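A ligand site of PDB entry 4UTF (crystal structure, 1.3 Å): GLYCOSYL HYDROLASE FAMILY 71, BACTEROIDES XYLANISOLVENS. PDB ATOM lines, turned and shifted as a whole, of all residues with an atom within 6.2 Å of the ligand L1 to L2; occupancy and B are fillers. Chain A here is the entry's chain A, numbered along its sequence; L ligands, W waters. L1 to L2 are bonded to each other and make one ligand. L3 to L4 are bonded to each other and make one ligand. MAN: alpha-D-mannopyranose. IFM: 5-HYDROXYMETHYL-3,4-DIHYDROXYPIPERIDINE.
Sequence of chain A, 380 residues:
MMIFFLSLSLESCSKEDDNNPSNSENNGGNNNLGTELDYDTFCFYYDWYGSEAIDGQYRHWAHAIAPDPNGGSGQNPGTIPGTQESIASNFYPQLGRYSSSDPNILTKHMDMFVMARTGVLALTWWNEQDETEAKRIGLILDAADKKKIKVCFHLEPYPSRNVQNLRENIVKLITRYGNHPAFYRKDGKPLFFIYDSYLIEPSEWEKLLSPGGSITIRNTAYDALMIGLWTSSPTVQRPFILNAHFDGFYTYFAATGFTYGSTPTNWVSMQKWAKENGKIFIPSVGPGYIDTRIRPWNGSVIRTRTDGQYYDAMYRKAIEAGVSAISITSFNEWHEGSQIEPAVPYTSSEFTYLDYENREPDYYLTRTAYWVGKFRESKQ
ND2 of Asn 298 lies within hydrogen-bond range of O4 of MAN L2 (3.0 Å).
An oxygen (O2) of MAN L2 sits at hydrogen-bond distance from the side-chain carboxylate (OE2) of Glu 336 (2.7 Å).
OH of Tyr 195 sits at hydrogen-bond distance from O3 of MAN L1 (2.7 Å).
The guanidinium group (NH2) of Arg 295 is in hydrogen-bond range of an oxygen (O6) of MAN L3 (3.0 Å).
An oxygen (O2) of MAN L2 lies within hydrogen-bond range of the guanidinium group of Arg 295, at 3.3 Å.
The side-chain hydroxyl (OH) of Tyr 198 is in hydrogen-bond range of an oxygen (O4) of MAN L1.
O4 of MAN L1 is in hydrogen-bond range of OD1 of Asp 196, 2.6 Å away.
The side-chain hydroxyl of Tyr 289 sits at hydrogen-bond distance from an oxygen (O3) of MAN L2 (2.8 Å).
N of IFM L4 lies within salt-bridge range of OE1 of Glu 336 (2.9 Å).
The side-chain carboxylate (OE2) of Glu 336 lies within hydrogen-bond range of the side-chain hydroxyl (OH) of Tyr 289, 3.5 Å away.
The side-chain carboxylate (OE2) of Glu 336 is in salt-bridge range of the guanidinium group (NH1) of Arg 295, at 2.9 Å.
OD2 of Asp 291 lies within hydrogen-bond range of OH of Tyr 289, at 2.6 Å.
The guanidinium group (NH1) of Arg 295 lies within salt-bridge range of the side-chain carboxylate (OD2) of Asp 291, at 2.9 Å.
The side-chain carboxylate of Asp 291 lies within hydrogen-bond range of the side-chain amide nitrogen of Asn 298 (2.9 Å).
The side-chain hydroxyl of Tyr 289 lies within hydrogen-bond range of the guanidinium group of Arg 295 (3.4 Å).
CZ of Phe 253 touches C4 of MAN L1 (3.7 Å).
Phe 258 touches the ligand L1 to L2.
Thr 259 touches the ligand L1 to L2.
CH2 of Trp 297 touches O6 of MAN L2, 3.9 Å away.
Hydrophobic or aromatic side chains within 4 Å of the ligand L1 to L2: Tyr 195, Tyr 198, Phe 253, Phe 258, Tyr 289 and Trp 297.
11 residues have an atom within 4 Å of the ligand L1 to L2: Tyr 195, Asp 196, Tyr 198, Phe 253, Phe 258, Thr 259, Tyr 289, Arg 295, Trp 297, Asn 298 and Glu 336.
Water W4 bridges O3 of MAN L2 and OE1 of Glu 336.
Water W3 lies within hydrogen-bond range of an oxygen (O6) of MAN L1 and the backbone carbonyl oxygen (O) of Phe 258.
Water W2 lies within hydrogen-bond range of O2 of MAN L2 (3.1 Å), NH2 of Arg 295 (3.2 Å) and O5 of MAN L3 (3.5 Å).
Water W8 lies within hydrogen-bond range of N of IFM L4 (2.7 Å) and OH of Tyr 195 (2.8 Å).
Water W5 bridges OD1 of Asn 298 (2.7 Å) and O4 of MAN L2 (3.5 Å).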
ATOM      1  N   PRO A  69      -1.570   4.436 -21.304  1.00  0.00           N
ATOM      2  CA  PRO A  69      -1.431   3.629 -22.545  1.00  0.00           C
ATOM      3  C   PRO A  69      -1.775   4.371 -23.864  1.00  0.00           C
ATOM      4  O   PRO A  69      -1.422   3.876 -24.935  1.00  0.00           O
ATOM      5  CB  PRO A  69      -2.374   2.441 -22.335  1.00  0.00           C
ATOM      6  CG  PRO A  69      -3.057   2.641 -21.024  1.00  0.00           C
ATOM      7  CD  PRO A  69      -2.616   3.925 -20.406  1.00  0.00           C
ATOM      8  N   TYR A 195      -7.206 -15.517 -12.785  1.00  0.00           N
ATOM      9  CA  TYR A 195      -7.315 -14.154 -13.271  1.00  0.00           C
ATOM     10  C   TYR A 195      -6.845 -14.052 -14.718  1.00  0.00           C
ATOM     11  O   TYR A 195      -5.857 -14.711 -15.100  1.00  0.00           O
ATOM     12  CB  TYR A 195      -6.583 -13.161 -12.360  1.00  0.00           C
ATOM     13  CG  TYR A 195      -6.884 -11.717 -12.762  1.00  0.00           C
ATOM     14  CD1 TYR A 195      -8.158 -11.188 -12.645  1.00  0.00           C
ATOM     15  CD2 TYR A 195      -5.905 -10.932 -13.346  1.00  0.00           C
ATOM     16  CE1 TYR A 195      -8.460  -9.902 -13.071  1.00  0.00           C
ATOM     17  CE2 TYR A 195      -6.201  -9.649 -13.784  1.00  0.00           C
ATOM     18  CZ  TYR A 195      -7.494  -9.155 -13.671  1.00  0.00           C
ATOM     19  OH  TYR A 195      -7.785  -7.879 -14.114  1.00  0.00           O
ATOM     20  N   ASP A 196      -7.542 -13.260 -15.535  1.00  0.00           N
ATOM     21  CA  ASP A 196      -7.165 -13.080 -16.944  1.00  0.00           C
ATOM     22  C   ASP A 196      -6.956 -14.412 -17.664  1.00  0.00           C
ATOM     23  O   ASP A 196      -6.012 -14.604 -18.418  1.00  0.00           O
ATOM     24  CB  ASP A 196      -6.013 -12.100 -17.114  1.00  0.00           C
ATOM     25  CG  ASP A 196      -6.440 -10.651 -16.918  1.00  0.00           C
ATOM     26  OD1 ASP A 196      -7.647 -10.399 -16.638  1.00  0.00           O
ATOM     27  OD2 ASP A 196      -5.574  -9.754 -17.049  1.00  0.00           O
ATOM     28  N   TYR A 198      -8.402 -15.609 -20.115  1.00  0.00           N
ATOM     29  CA  TYR A 198      -8.478 -15.470 -21.559  1.00  0.00           C
ATOM     30  C   TYR A 198      -7.118 -15.331 -22.230  1.00  0.00           C
ATOM     31  O   TYR A 198      -7.033 -15.464 -23.442  1.00  0.00           O
ATOM     32  CB  TYR A 198      -9.340 -14.263 -21.956  1.00  0.00           C
ATOM     33  CG  TYR A 198      -8.822 -12.930 -21.450  1.00  0.00           C
ATOM     34  CD1 TYR A 198      -7.850 -12.221 -22.137  1.00  0.00           C
ATOM     35  CD2 TYR A 198      -9.293 -12.379 -20.262  1.00  0.00           C
ATOM     36  CE1 TYR A 198      -7.387 -11.003 -21.672  1.00  0.00           C
ATOM     37  CE2 TYR A 198      -8.829 -11.161 -19.797  1.00  0.00           C
ATOM     38  CZ  TYR A 198      -7.867 -10.479 -20.493  1.00  0.00           C
ATOM     39  OH  TYR A 198      -7.372  -9.271 -20.091  1.00  0.00           O
ATOM     40  N   LEU A 229     -12.328 -16.278 -15.688  1.00  0.00           N
ATOM     41  CA  LEU A 229     -12.810 -14.901 -15.675  1.00  0.00           C
ATOM     42  C   LEU A 229     -13.713 -14.615 -16.882  1.00  0.00           C
ATOM     43  O   LEU A 229     -13.246 -14.588 -18.025  1.00  0.00           O
ATOM     44  CB  LEU A 229     -11.625 -13.932 -15.699  1.00  0.00           C
ATOM     45  CG  LEU A 229     -11.985 -12.450 -15.579  1.00  0.00           C
ATOM     46  CD1 LEU A 229     -12.530 -12.131 -14.209  1.00  0.00           C
ATOM     47  CD2 LEU A 229     -10.822 -11.551 -15.890  1.00  0.00           C
ATOM     48  N   THR A 231     -15.268 -12.020 -19.084  1.00  0.00           N
ATOM     49  CA  THR A 231     -15.038 -10.605 -19.386  1.00  0.00           C
ATOM     50  C   THR A 231     -16.138 -10.033 -20.281  1.00  0.00           C
ATOM     51  O   THR A 231     -16.994  -9.278 -19.833  1.00  0.00           O
ATOM     52  CB  THR A 231     -13.647 -10.379 -20.015  1.00  0.00           C
ATOM     53  OG1 THR A 231     -13.483 -11.268 -21.112  1.00  0.00           O
ATOM     54  CG2 THR A 231     -12.536 -10.615 -19.007  1.00  0.00           C
ATOM     55  N   TYR A 252     -14.767 -10.490 -11.307  1.00  0.00           N
ATOM     56  CA  TYR A 252     -13.743  -9.688 -10.613  1.00  0.00           C
ATOM     57  C   TYR A 252     -14.018  -8.179 -10.446  1.00  0.00           C
ATOM     58  O   TYR A 252     -14.023  -7.675  -9.332  1.00  0.00           O
ATOM     59  CB  TYR A 252     -12.296  -9.869 -11.183  1.00  0.00           C
ATOM     60  CG  TYR A 252     -11.336  -9.212 -10.220  1.00  0.00           C
ATOM     61  CD1 TYR A 252     -10.983  -9.816  -9.013  1.00  0.00           C
ATOM     62  CD2 TYR A 252     -10.859  -7.939 -10.466  1.00  0.00           C
ATOM     63  CE1 TYR A 252     -10.215  -9.175  -8.070  1.00  0.00           C
ATOM     64  CE2 TYR A 252     -10.092  -7.279  -9.510  1.00  0.00           C
ATOM     65  CZ  TYR A 252      -9.760  -7.901  -8.319  1.00  0.00           C
ATOM     66  OH  TYR A 252      -9.030  -7.193  -7.374  1.00  0.00           O
ATOM     67  N   PHE A 253     -14.194  -7.438 -11.539  1.00  0.00           N
ATOM     68  CA  PHE A 253     -14.048  -5.993 -11.465  1.00  0.00           C
ATOM     69  C   PHE A 253     -15.098  -5.372 -10.567  1.00  0.00           C
ATOM     70  O   PHE A 253     -16.292  -5.614 -10.715  1.00  0.00           O
ATOM     71  CB  PHE A 253     -14.055  -5.372 -12.870  1.00  0.00           C
ATOM     72  CG  PHE A 253     -13.068  -6.051 -13.759  1.00  0.00           C
ATOM     73  CD1 PHE A 253     -11.709  -5.864 -13.545  1.00  0.00           C
ATOM     74  CD2 PHE A 253     -13.450  -6.969 -14.715  1.00  0.00           C
ATOM     75  CE1 PHE A 253     -10.770  -6.553 -14.265  1.00  0.00           C
ATOM     76  CE2 PHE A 253     -12.497  -7.663 -15.435  1.00  0.00           C
ATOM     77  CZ  PHE A 253     -11.167  -7.473 -15.212  1.00  0.00           C
ATOM     78  N   PHE A 258     -17.383  -1.819 -16.334  1.00  0.00           N
ATOM     79  CA  PHE A 258     -16.023  -1.906 -16.867  1.00  0.00           C
ATOM     80  C   PHE A 258     -15.919  -2.981 -17.956  1.00  0.00           C
ATOM     81  O   PHE A 258     -15.256  -2.782 -18.981  1.00  0.00           O
ATOM     82  CB  PHE A 258     -14.998  -2.103 -15.748  1.00  0.00           C
ATOM     83  CG  PHE A 258     -13.588  -2.158 -16.237  1.00  0.00           C
ATOM     84  CD1 PHE A 258     -13.004  -1.056 -16.818  1.00  0.00           C
ATOM     85  CD2 PHE A 258     -12.857  -3.332 -16.149  1.00  0.00           C
ATOM     86  CE1 PHE A 258     -11.719  -1.107 -17.289  1.00  0.00           C
ATOM     87  CE2 PHE A 258     -11.573  -3.388 -16.637  1.00  0.00           C
ATOM     88  CZ  PHE A 258     -11.009  -2.280 -17.204  1.00  0.00           C
ATOM     89  N   THR A 259     -16.589  -4.113 -17.732  1.00  0.00           N
ATOM     90  CA  THR A 259     -16.759  -5.149 -18.732  1.00  0.00           C
ATOM     91  C   THR A 259     -18.236  -5.542 -18.766  1.00  0.00           C
ATOM     92  O   THR A 259     -19.008  -5.188 -17.880  1.00  0.00           O
ATOM     93  CB  THR A 259     -15.972  -6.422 -18.371  1.00  0.00           C
ATOM     94  OG1 THR A 259     -16.456  -6.906 -17.119  1.00  0.00           O
ATOM     95  CG2 THR A 259     -14.471  -6.165 -18.305  1.00  0.00           C
ATOM     96  N   TYR A 289     -14.574   1.974  -6.687  1.00  0.00           N
ATOM     97  CA  TYR A 289     -13.321   1.815  -7.413  1.00  0.00           C
ATOM     98  C   TYR A 289     -12.677   3.179  -7.590  1.00  0.00           C
ATOM     99  O   TYR A 289     -13.337   4.144  -8.033  1.00  0.00           O
ATOM    100  CB  TYR A 289     -13.552   1.172  -8.790  1.00  0.00           C
ATOM    101  CG  TYR A 289     -12.258   0.817  -9.497  1.00  0.00           C
ATOM    102  CD1 TYR A 289     -11.577   1.761 -10.245  1.00  0.00           C
ATOM    103  CD2 TYR A 289     -11.705  -0.451  -9.396  1.00  0.00           C
ATOM    104  CE1 TYR A 289     -10.347   1.468 -10.858  1.00  0.00           C
ATOM    105  CE2 TYR A 289     -10.511  -0.762 -10.016  1.00  0.00           C
ATOM    106  CZ  TYR A 289      -9.827   0.192 -10.755  1.00  0.00           C
ATOM    107  OH  TYR A 289      -8.628  -0.151 -11.360  1.00  0.00           O
ATOM    108  N   ASP A 291      -8.391   4.239  -8.746  1.00  0.00           N
ATOM    109  CA  ASP A 291      -6.997   3.846  -8.832  1.00  0.00           C
ATOM    110  C   ASP A 291      -6.103   4.973  -9.327  1.00  0.00           C
ATOM    111  O   ASP A 291      -5.002   4.722  -9.811  1.00  0.00           O
ATOM    112  CB  ASP A 291      -6.851   2.597  -9.739  1.00  0.00           C
ATOM    113  CG  ASP A 291      -7.154   2.865 -11.197  1.00  0.00           C
ATOM    114  OD1 ASP A 291      -7.461   4.013 -11.572  1.00  0.00           O
ATOM    115  OD2 ASP A 291      -7.108   1.891 -12.004  1.00  0.00           O
ATOM    116  N   ARG A 295      -2.739   5.163 -11.403  1.00  0.00           N
ATOM    117  CA  ARG A 295      -3.149   5.235 -12.819  1.00  0.00           C
ATOM    118  C   ARG A 295      -3.895   6.542 -13.038  1.00  0.00           C
ATOM    119  O   ARG A 295      -5.127   6.550 -13.155  1.00  0.00           O
ATOM    120  CB  ARG A 295      -4.023   4.029 -13.226  1.00  0.00           C
ATOM    121  CG  ARG A 295      -3.378   2.687 -12.877  1.00  0.00           C
ATOM    122  CD  ARG A 295      -4.102   1.513 -13.493  1.00  0.00           C
ATOM    123  NE  ARG A 295      -3.556   0.226 -13.073  1.00  0.00           N
ATOM    124  CZ  ARG A 295      -4.101  -0.599 -12.181  1.00  0.00           C
ATOM    125  NH1 ARG A 295      -5.244  -0.311 -11.580  1.00  0.00           N
ATOM    126  NH2 ARG A 295      -3.489  -1.742 -11.847  1.00  0.00           N
ATOM    127  N   TRP A 297      -4.460   8.536 -15.359  1.00  0.00           N
ATOM    128  CA  TRP A 297      -5.216   8.574 -16.615  1.00  0.00           C
ATOM    129  C   TRP A 297      -6.516   7.777 -16.602  1.00  0.00           C
ATOM    130  O   TRP A 297      -7.251   7.794 -17.598  1.00  0.00           O
ATOM    131  CB  TRP A 297      -4.289   8.068 -17.751  1.00  0.00           C
ATOM    132  CG  TRP A 297      -3.527   6.851 -17.355  1.00  0.00           C
ATOM    133  CD1 TRP A 297      -2.263   6.812 -16.811  1.00  0.00           C
ATOM    134  CD2 TRP A 297      -3.968   5.484 -17.427  1.00  0.00           C
ATOM    135  NE1 TRP A 297      -1.918   5.519 -16.530  1.00  0.00           N
ATOM    136  CE2 TRP A 297      -2.937   4.682 -16.890  1.00  0.00           C
ATOM    137  CE3 TRP A 297      -5.143   4.868 -17.882  1.00  0.00           C
ATOM    138  CZ2 TRP A 297      -3.028   3.296 -16.826  1.00  0.00           C
ATOM    139  CZ3 TRP A 297      -5.241   3.479 -17.797  1.00  0.00           C
ATOM    140  CH2 TRP A 297      -4.192   2.714 -17.281  1.00  0.00           C
ATOM    141  N   ASN A 298      -6.785   7.042 -15.524  1.00  0.00           N
ATOM    142  CA  ASN A 298      -7.892   6.067 -15.516  1.00  0.00           C
ATOM    143  C   ASN A 298      -9.139   6.559 -14.767  1.00  0.00           C
ATOM    144  O   ASN A 298      -9.920   5.758 -14.282  1.00  0.00           O
ATOM    145  CB  ASN A 298      -7.381   4.736 -14.923  1.00  0.00           C
ATOM    146  CG  ASN A 298      -8.148   3.526 -15.412  1.00  0.00           C
ATOM    147  OD1 ASN A 298      -8.650   3.505 -16.565  1.00  0.00           O
ATOM    148  ND2 ASN A 298      -8.222   2.487 -14.573  1.00  0.00           N
ATOM    149  N   VAL A 301     -12.922   5.168 -14.824  1.00  0.00           N
ATOM    150  CA  VAL A 301     -13.309   3.947 -14.144  1.00  0.00           C
ATOM    151  C   VAL A 301     -13.691   4.224 -12.663  1.00  0.00           C
ATOM    152  O   VAL A 301     -14.172   3.330 -11.968  1.00  0.00           O
ATOM    153  CB  VAL A 301     -12.200   2.870 -14.290  1.00  0.00           C
ATOM    154  CG1 VAL A 301     -12.632   1.513 -13.787  1.00  0.00           C
ATOM    155  CG2 VAL A 301     -11.800   2.739 -15.752  1.00  0.00           C
ATOM    156  N   GLU A 336      -6.495  -0.002  -5.956  1.00  0.00           N
ATOM    157  CA  GLU A 336      -7.678   0.123  -6.783  1.00  0.00           C
ATOM    158  C   GLU A 336      -8.893   0.646  -6.031  1.00  0.00           C
ATOM    159  O   GLU A 336      -9.945   0.866  -6.633  1.00  0.00           O
ATOM    160  CB  GLU A 336      -7.947  -1.193  -7.503  1.00  0.00           C
ATOM    161  CG  GLU A 336      -6.858  -1.491  -8.527  1.00  0.00           C
ATOM    162  CD  GLU A 336      -7.065  -2.710  -9.390  1.00  0.00           C
ATOM    163  OE1 GLU A 336      -7.818  -3.640  -8.991  1.00  0.00           O
ATOM    164  OE2 GLU A 336      -6.435  -2.737 -10.492  1.00  0.00           O
HETATM  165  C1  MAN L   1      -7.434  -4.412 -18.509  1.00  0.00           C
HETATM  166  C2  MAN L   1      -6.756  -5.152 -17.351  1.00  0.00           C
HETATM  167  C3  MAN L   1      -6.935  -6.647 -17.466  1.00  0.00           C
HETATM  168  C4  MAN L   1      -8.420  -6.976 -17.640  1.00  0.00           C
HETATM  169  C5  MAN L   1      -9.049  -6.155 -18.770  1.00  0.00           C
HETATM  170  C6  MAN L   1     -10.554  -6.392 -18.897  1.00  0.00           C
HETATM  171  O1  MAN L   1      -6.738  -4.678 -19.716  1.00  0.00           O
HETATM  172  O2  MAN L   1      -7.356  -4.730 -16.128  1.00  0.00           O
HETATM  173  O3  MAN L   1      -6.347  -7.340 -16.352  1.00  0.00           O
HETATM  174  O4  MAN L   1      -8.622  -8.353 -17.935  1.00  0.00           O
HETATM  175  O5  MAN L   1      -8.830  -4.758 -18.581  1.00  0.00           O
HETATM  176  O6  MAN L   1     -11.063  -5.816 -20.065  1.00  0.00           O
HETATM  177  C1  MAN L   2      -6.558  -3.836 -15.337  1.00  0.00           C
HETATM  178  C2  MAN L   2      -7.332  -3.570 -14.057  1.00  0.00           C
HETATM  179  C3  MAN L   2      -8.508  -2.602 -14.245  1.00  0.00           C
HETATM  180  C4  MAN L   2      -8.047  -1.260 -14.828  1.00  0.00           C
HETATM  181  C5  MAN L   2      -7.280  -1.597 -16.109  1.00  0.00           C
HETATM  182  C6  MAN L   2      -6.598  -0.339 -16.626  1.00  0.00           C
HETATM  183  O2  MAN L   2      -6.406  -2.979 -13.196  1.00  0.00           O
HETATM  184  O3  MAN L   2      -9.230  -2.371 -13.029  1.00  0.00           O
HETATM  185  O4  MAN L   2      -9.136  -0.356 -15.107  1.00  0.00           O
HETATM  186  O5  MAN L   2      -6.249  -2.578 -15.895  1.00  0.00           O
HETATM  187  O6  MAN L   2      -6.146  -0.561 -17.945  1.00  0.00           O
HETATM  188  C1  MAN L   3      -1.776  -5.647 -11.086  1.00  0.00           C
HETATM  189  C2  MAN L   3      -0.284  -5.963 -11.064  1.00  0.00           C
HETATM  190  C3  MAN L   3       0.339  -5.642  -9.706  1.00  0.00           C
HETATM  191  C4  MAN L   3       0.018  -4.199  -9.298  1.00  0.00           C
HETATM  192  C5  MAN L   3      -1.520  -4.044  -9.341  1.00  0.00           C
HETATM  193  C6  MAN L   3      -1.959  -2.610  -8.998  1.00  0.00           C
HETATM  194  O2  MAN L   3       0.309  -5.176 -12.085  1.00  0.00           O
HETATM  195  O3  MAN L   3       1.768  -5.822  -9.736  1.00  0.00           O
HETATM  196  O4  MAN L   3       0.490  -3.950  -7.980  1.00  0.00           O
HETATM  197  O5  MAN L   3      -1.998  -4.314 -10.652  1.00  0.00           O
HETATM  198  O6  MAN L   3      -3.375  -2.483  -8.954  1.00  0.00           O
HETATM  199  O4  IFM L   4      -3.716  -9.046 -11.095  1.00  0.00           O
HETATM  200  C4  IFM L   4      -4.321  -8.116 -10.159  1.00  0.00           C
HETATM  201  C3  IFM L   4      -3.858  -6.709 -10.512  1.00  0.00           C
HETATM  202  O3  IFM L   4      -2.424  -6.656 -10.304  1.00  0.00           O
HETATM  203  C2  IFM L   4      -4.521  -5.601  -9.672  1.00  0.00           C
HETATM  204  N   IFM L   4      -5.970  -5.791  -9.730  1.00  0.00           N
HETATM  205  C1  IFM L   4      -6.436  -7.106  -9.265  1.00  0.00           C
HETATM  206  C5  IFM L   4      -5.850  -8.188 -10.187  1.00  0.00           C
HETATM  207  C6  IFM L   4      -6.406  -9.571  -9.773  1.00  0.00           C
HETATM  208  O6  IFM L   4      -6.069  -9.904  -8.417  1.00  0.00           O
HETATM  209  O   HOH W   1      -3.976  -6.557 -14.901  1.00  0.00           O
HETATM  210  O   HOH W   2      -3.719  -4.373 -13.676  1.00  0.00           O
HETATM  211  O   HOH W   3     -12.508  -3.420 -20.056  1.00  0.00           O
HETATM  212  O   HOH W   4      -9.555  -4.338 -11.121  1.00  0.00           O
HETATM  213  O   HOH W   5      -9.411   1.390 -18.091  1.00  0.00           O
HETATM  214  O   HOH W   6     -13.117  -7.223 -21.686  1.00  0.00           O
HETATM  215  O   HOH W   7      -4.028  -5.185 -19.684  1.00  0.00           O
HETATM  216  O   HOH W   8      -7.613  -6.100 -11.905  1.00  0.00           O
HETATM  217  O   HOH W   9      -6.851  -2.899 -21.885  1.00  0.00           O
